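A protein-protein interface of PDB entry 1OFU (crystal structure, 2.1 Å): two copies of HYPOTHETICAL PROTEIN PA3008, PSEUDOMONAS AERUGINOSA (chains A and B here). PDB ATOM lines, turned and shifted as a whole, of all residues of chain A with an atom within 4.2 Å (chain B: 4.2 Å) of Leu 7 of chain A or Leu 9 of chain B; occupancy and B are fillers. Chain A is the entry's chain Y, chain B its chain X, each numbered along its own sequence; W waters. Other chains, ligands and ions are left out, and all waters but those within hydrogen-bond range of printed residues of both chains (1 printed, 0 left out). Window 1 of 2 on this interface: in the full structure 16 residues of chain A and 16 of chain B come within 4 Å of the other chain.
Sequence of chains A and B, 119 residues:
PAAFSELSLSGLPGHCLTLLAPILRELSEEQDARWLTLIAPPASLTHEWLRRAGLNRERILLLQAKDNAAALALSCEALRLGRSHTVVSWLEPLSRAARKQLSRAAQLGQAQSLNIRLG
Of the printed residues of chain B, Leu 7 of chain A touches Ser 8 and Leu 9.
Printed residues of chain B within 4 Å of Glu 6 of chain A: Ser 8, Leu 9 and Ser 10.
Of the printed residues of chain A, Leu 19 of chain B touches Ile 23.
The nearest printed residue of chain B that does not touch Leu 7 of chain A is Leu 7 of chain B (4.7 Å).
The nearest printed residue of chain B that does not touch Glu 6 of chain A is Leu 19 of chain B (5.7 Å).
The guanidinium group (NH2) of Arg 117 of chain B is in hydrogen-bond range of the side-chain hydroxyl (OG) of Ser 8 of chain B, at 2.8 Å.
The backbone carbonyl oxygen (O) of Leu 9 of chain B is in hydrogen-bond range of the side-chain sulfur (SG) of Cys 16 of chain B, at 3.8 Å.
NH2 of Arg 117 of chain A is in salt-bridge range of OE1 of Glu 6 of chain A (3.2 Å).
N of Leu 7 of chain A lies within hydrogen-bond range of O of Asn 115 of chain A (2.8 Å).
The backbone carbonyl oxygen (O) of Leu 7 of chain A lies within hydrogen-bond range of the backbone NH (N) of Arg 117 of chain A (2.9 Å).
The backbone NH (N) of Leu 9 of chain A is in hydrogen-bond range of the backbone carbonyl oxygen (O) of Arg 117 of chain A (2.9 Å).
Of the 8 printed residues of chain A, 5 touch a printed residue of chain B.
Printed residues of chain A that touch a printed residue of chain B: Glu 6, Leu 7, Ser 8, Leu 9 and Ile 23.
Of the 9 printed residues of chain B, 5 touch a printed residue of chain A.
Hydrophobic or aromatic side chains of chain B that line the printed part of chain A: Leu 7 and Leu 9.
Among the printed residues, 9 pairs touch across the chains.
Among the printed residues, no Asp or Glu carboxylate lies within 4 Å of a Lys or Arg side-chain nitrogen of the other chain.
Water W1 lies within hydrogen-bond range of OG of Ser 10 of chain B (2.5 Å) and OE1 of Glu 6 of chain A (2.7 Å).
Glu 6 of chain A touches Ser 8 of chain B.
Glu 6 of chain A touches Leu 9 of chain B (O to CA, 3.4 Å).
Leu 7 of chain A touches Ser 8 of chain B (CA to O, 3.3 Å).
Leu 7 of chain A touches Leu 9 of chain B (CB to CD2, 3.7 Å).
Leu 7 of chain B touches Ser 8 of chain A (CA to O, 3.3 Å).
CD2 of Leu 9 of chain A touches CG of Leu 7 of chain B (3.6 Å).
CG1 of Ile 23 of chain A touches O of Leu 19 of chain B (3.8 Å).
The backbone carbonyl oxygen of Ser 8 of chain A sits at hydrogen-bond distance from the backbone NH of Ser 8 of chain B (2.8 Å).
The backbone carbonyl oxygen (O) of Glu 6 of chain A is in hydrogen-bond range of the backbone NH (N) of Ser 10 of chain B.
Leu 7 of chain A touches Ser 8 of chain B, and with the chains exchanged Ser 8 of chain A touches Leu 7 of chain B.
Leu 7 of chain A touches Leu 9 of chain B, and with the chains exchanged Leu 9 of chain A touches Leu 7 of chain B.
Ser 8 of chain A touches its own counterpart, Ser 8 of chain B.
Positions printed for both chains: 7, 8, 9 and 117.
Of the 9 pairs that touch across the chains among the printed residues, 5 have their exchanged pair printed and touching as well.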
ATOM      1  N   GLU A   6      30.727  -3.606   8.769  1.00  0.00           N
ATOM      2  CA  GLU A   6      29.444  -3.409   8.132  1.00  0.00           C
ATOM      3  C   GLU A   6      28.548  -4.589   8.430  1.00  0.00           C
ATOM      4  O   GLU A   6      28.966  -5.747   8.339  1.00  0.00           O
ATOM      5  CB  GLU A   6      29.590  -3.230   6.624  1.00  0.00           C
ATOM      6  CG  GLU A   6      28.256  -2.994   5.932  1.00  0.00           C
ATOM      7  CD  GLU A   6      28.411  -2.589   4.480  1.00  0.00           C
ATOM      8  OE1 GLU A   6      28.896  -3.411   3.677  1.00  0.00           O
ATOM      9  OE2 GLU A   6      28.046  -1.442   4.143  1.00  0.00           O
ATOM     10  N   LEU A   7      27.318  -4.275   8.815  1.00  0.00           N
ATOM     11  CA  LEU A   7      26.340  -5.291   9.134  1.00  0.00           C
ATOM     12  C   LEU A   7      25.169  -5.170   8.182  1.00  0.00           C
ATOM     13  O   LEU A   7      24.592  -4.087   8.014  1.00  0.00           O
ATOM     14  CB  LEU A   7      25.875  -5.132  10.581  1.00  0.00           C
ATOM     15  CG  LEU A   7      24.824  -6.144  11.048  1.00  0.00           C
ATOM     16  CD1 LEU A   7      24.938  -6.343  12.540  1.00  0.00           C
ATOM     17  CD2 LEU A   7      23.441  -5.665  10.673  1.00  0.00           C
ATOM     18  N   SER A   8      24.829  -6.282   7.541  1.00  0.00           N
ATOM     19  CA  SER A   8      23.716  -6.302   6.610  1.00  0.00           C
ATOM     20  C   SER A   8      22.679  -7.295   7.101  1.00  0.00           C
ATOM     21  O   SER A   8      23.017  -8.385   7.557  1.00  0.00           O
ATOM     22  CB  SER A   8      24.203  -6.704   5.226  1.00  0.00           C
ATOM     23  OG  SER A   8      25.336  -5.937   4.865  1.00  0.00           O
ATOM     24  N   LEU A   9      21.415  -6.902   7.023  1.00  0.00           N
ATOM     25  CA  LEU A   9      20.318  -7.752   7.451  1.00  0.00           C
ATOM     26  C   LEU A   9      19.314  -7.828   6.316  1.00  0.00           C
ATOM     27  O   LEU A   9      18.865  -6.800   5.802  1.00  0.00           O
ATOM     28  CB  LEU A   9      19.647  -7.171   8.690  1.00  0.00           C
ATOM     29  CG  LEU A   9      20.426  -7.227  10.003  1.00  0.00           C
ATOM     30  CD1 LEU A   9      19.748  -6.334  11.032  1.00  0.00           C
ATOM     31  CD2 LEU A   9      20.493  -8.669  10.498  1.00  0.00           C
ATOM     32  N   ILE A  23      22.008  -5.809  19.226  1.00  0.00           N
ATOM     33  CA  ILE A  23      23.313  -5.226  18.947  1.00  0.00           C
ATOM     34  C   ILE A  23      23.343  -3.768  19.393  1.00  0.00           C
ATOM     35  O   ILE A  23      24.307  -3.307  20.015  1.00  0.00           O
ATOM     36  CB  ILE A  23      23.633  -5.318  17.442  1.00  0.00           C
ATOM     37  CG1 ILE A  23      23.790  -6.788  17.047  1.00  0.00           C
ATOM     38  CG2 ILE A  23      24.885  -4.521  17.122  1.00  0.00           C
ATOM     39  CD1 ILE A  23      23.996  -7.010  15.577  1.00  0.00           C
ATOM     40  N   ASN A 115      28.538   0.441   9.793  1.00  0.00           N
ATOM     41  CA  ASN A 115      27.500   0.784   8.848  1.00  0.00           C
ATOM     42  C   ASN A 115      26.510  -0.361   8.811  1.00  0.00           C
ATOM     43  O   ASN A 115      26.895  -1.534   8.836  1.00  0.00           O
ATOM     44  CB  ASN A 115      28.058   1.014   7.448  1.00  0.00           C
ATOM     45  CG  ASN A 115      27.053   1.698   6.545  1.00  0.00           C
ATOM     46  OD1 ASN A 115      26.568   2.782   6.864  1.00  0.00           O
ATOM     47  ND2 ASN A 115      26.726   1.071   5.417  1.00  0.00           N
ATOM     48  N   ILE A 116      25.231  -0.013   8.755  1.00  0.00           N
ATOM     49  CA  ILE A 116      24.179  -1.003   8.723  1.00  0.00           C
ATOM     50  C   ILE A 116      23.346  -0.860   7.461  1.00  0.00           C
ATOM     51  O   ILE A 116      23.018   0.246   7.041  1.00  0.00           O
ATOM     52  CB  ILE A 116      23.295  -0.879   9.988  1.00  0.00           C
ATOM     53  CG1 ILE A 116      24.157  -1.203  11.213  1.00  0.00           C
ATOM     54  CG2 ILE A 116      22.068  -1.806   9.892  1.00  0.00           C
ATOM     55  CD1 ILE A 116      23.447  -1.068  12.535  1.00  0.00           C
ATOM     56  N   ARG A 117      23.030  -1.997   6.852  1.00  0.00           N
ATOM     57  CA  ARG A 117      22.237  -2.039   5.631  1.00  0.00           C
ATOM     58  C   ARG A 117      21.061  -2.973   5.851  1.00  0.00           C
ATOM     59  O   ARG A 117      21.245  -4.129   6.227  1.00  0.00           O
ATOM     60  CB  ARG A 117      23.078  -2.568   4.476  1.00  0.00           C
ATOM     61  CG  ARG A 117      24.272  -1.710   4.124  1.00  0.00           C
ATOM     62  CD  ARG A 117      25.294  -2.520   3.339  1.00  0.00           C
ATOM     63  NE  ARG A 117      24.685  -3.294   2.261  1.00  0.00           N
ATOM     64  CZ  ARG A 117      25.364  -4.054   1.406  1.00  0.00           C
ATOM     65  NH1 ARG A 117      24.722  -4.726   0.459  1.00  0.00           N
ATOM     66  NH2 ARG A 117      26.686  -4.139   1.491  1.00  0.00           N
ATOM     67  N   LEU B   7      21.977 -12.548   7.900  1.00  0.00           N
ATOM     68  CA  LEU B   7      22.778 -11.530   8.550  1.00  0.00           C
ATOM     69  C   LEU B   7      24.200 -11.677   8.029  1.00  0.00           C
ATOM     70  O   LEU B   7      24.764 -12.775   8.053  1.00  0.00           O
ATOM     71  CB  LEU B   7      22.738 -11.739  10.062  1.00  0.00           C
ATOM     72  CG  LEU B   7      23.442 -10.722  10.971  1.00  0.00           C
ATOM     73  CD1 LEU B   7      22.936 -10.911  12.387  1.00  0.00           C
ATOM     74  CD2 LEU B   7      24.952 -10.890  10.912  1.00  0.00           C
ATOM     75  N   SER B   8      24.766 -10.571   7.551  1.00  0.00           N
ATOM     76  CA  SER B   8      26.122 -10.555   7.009  1.00  0.00           C
ATOM     77  C   SER B   8      26.989  -9.579   7.785  1.00  0.00           C
ATOM     78  O   SER B   8      26.546  -8.476   8.127  1.00  0.00           O
ATOM     79  CB  SER B   8      26.115 -10.121   5.543  1.00  0.00           C
ATOM     80  OG  SER B   8      25.322 -10.983   4.753  1.00  0.00           O
ATOM     81  N   LEU B   9      28.227  -9.985   8.048  1.00  0.00           N
ATOM     82  CA  LEU B   9      29.168  -9.142   8.766  1.00  0.00           C
ATOM     83  C   LEU B   9      30.479  -9.012   7.999  1.00  0.00           C
ATOM     84  O   LEU B   9      31.101 -10.012   7.650  1.00  0.00           O
ATOM     85  CB  LEU B   9      29.438  -9.709  10.160  1.00  0.00           C
ATOM     86  CG  LEU B   9      28.348  -9.459  11.205  1.00  0.00           C
ATOM     87  CD1 LEU B   9      28.740 -10.105  12.523  1.00  0.00           C
ATOM     88  CD2 LEU B   9      28.152  -7.956  11.394  1.00  0.00           C
ATOM     89  N   SER B  10      30.884  -7.774   7.728  1.00  0.00           N
ATOM     90  CA  SER B  10      32.129  -7.506   7.016  1.00  0.00           C
ATOM     91  C   SER B  10      33.073  -6.758   7.940  1.00  0.00           C
ATOM     92  O   SER B  10      32.647  -5.866   8.672  1.00  0.00           O
ATOM     93  CB  SER B  10      31.866  -6.649   5.775  1.00  0.00           C
ATOM     94  OG  SER B  10      30.960  -7.280   4.890  1.00  0.00           O
ATOM     95  N   CYS B  16      33.727  -8.991  13.747  1.00  0.00           N
ATOM     96  CA  CYS B  16      32.534  -9.718  13.342  1.00  0.00           C
ATOM     97  C   CYS B  16      32.021 -10.619  14.463  1.00  0.00           C
ATOM     98  O   CYS B  16      30.823 -10.665  14.726  1.00  0.00           O
ATOM     99  CB  CYS B  16      32.830 -10.548  12.090  1.00  0.00           C
ATOM    100  SG  CYS B  16      33.363  -9.557  10.652  1.00  0.00           S
ATOM    101  N   LEU B  19      30.390  -8.563  17.305  1.00  0.00           N
ATOM    102  CA  LEU B  19      29.076  -8.067  16.914  1.00  0.00           C
ATOM    103  C   LEU B  19      28.026  -9.172  16.896  1.00  0.00           C
ATOM    104  O   LEU B  19      26.870  -8.949  17.246  1.00  0.00           O
ATOM    105  CB  LEU B  19      29.160  -7.407  15.532  1.00  0.00           C
ATOM    106  CG  LEU B  19      29.941  -6.087  15.500  1.00  0.00           C
ATOM    107  CD1 LEU B  19      30.135  -5.616  14.061  1.00  0.00           C
ATOM    108  CD2 LEU B  19      29.189  -5.048  16.323  1.00  0.00           C
ATOM    109  N   LEU B  20      28.443 -10.367  16.495  1.00  0.00           N
ATOM    110  CA  LEU B  20      27.551 -11.518  16.421  1.00  0.00           C
ATOM    111  C   LEU B  20      27.105 -12.014  17.796  1.00  0.00           C
ATOM    112  O   LEU B  20      25.952 -12.394  17.974  1.00  0.00           O
ATOM    113  CB  LEU B  20      28.248 -12.653  15.659  1.00  0.00           C
ATOM    114  CG  LEU B  20      27.597 -14.040  15.626  1.00  0.00           C
ATOM    115  CD1 LEU B  20      26.169 -13.948  15.107  1.00  0.00           C
ATOM    116  CD2 LEU B  20      28.430 -14.951  14.745  1.00  0.00           C
ATOM    117  N   ARG B 117      26.563 -14.840   7.273  1.00  0.00           N
ATOM    118  CA  ARG B 117      27.683 -14.771   6.344  1.00  0.00           C
ATOM    119  C   ARG B 117      28.777 -13.919   6.970  1.00  0.00           C
ATOM    120  O   ARG B 117      28.602 -12.714   7.134  1.00  0.00           O
ATOM    121  CB  ARG B 117      27.250 -14.119   5.032  1.00  0.00           C
ATOM    122  CG  ARG B 117      26.237 -14.905   4.226  1.00  0.00           C
ATOM    123  CD  ARG B 117      25.473 -13.972   3.304  1.00  0.00           C
ATOM    124  NE  ARG B 117      26.357 -13.234   2.408  1.00  0.00           N
ATOM    125  CZ  ARG B 117      26.039 -12.077   1.835  1.00  0.00           C
ATOM    126  NH1 ARG B 117      26.904 -11.475   1.029  1.00  0.00           N
ATOM    127  NH2 ARG B 117      24.864 -11.511   2.081  1.00  0.00           N
ATOM    128  N   LEU B 118      29.900 -14.542   7.315  1.00  0.00           N
ATOM    129  CA  LEU B 118      31.016 -13.820   7.920  1.00  0.00           C
ATOM    130  C   LEU B 118      32.079 -13.441   6.890  1.00  0.00           C
ATOM    131  O   LEU B 118      33.097 -12.836   7.293  1.00  0.00           O
ATOM    132  CB  LEU B 118      31.659 -14.663   9.023  1.00  0.00           C
ATOM    133  CG  LEU B 118      30.804 -14.949  10.259  1.00  0.00           C
ATOM    134  CD1 LEU B 118      31.612 -15.765  11.257  1.00  0.00           C
ATOM    135  CD2 LEU B 118      30.351 -13.638  10.888  1.00  0.00           C
HETATM  136  O   HOH W   1      29.072  -6.071   3.742  1.00  0.00           O
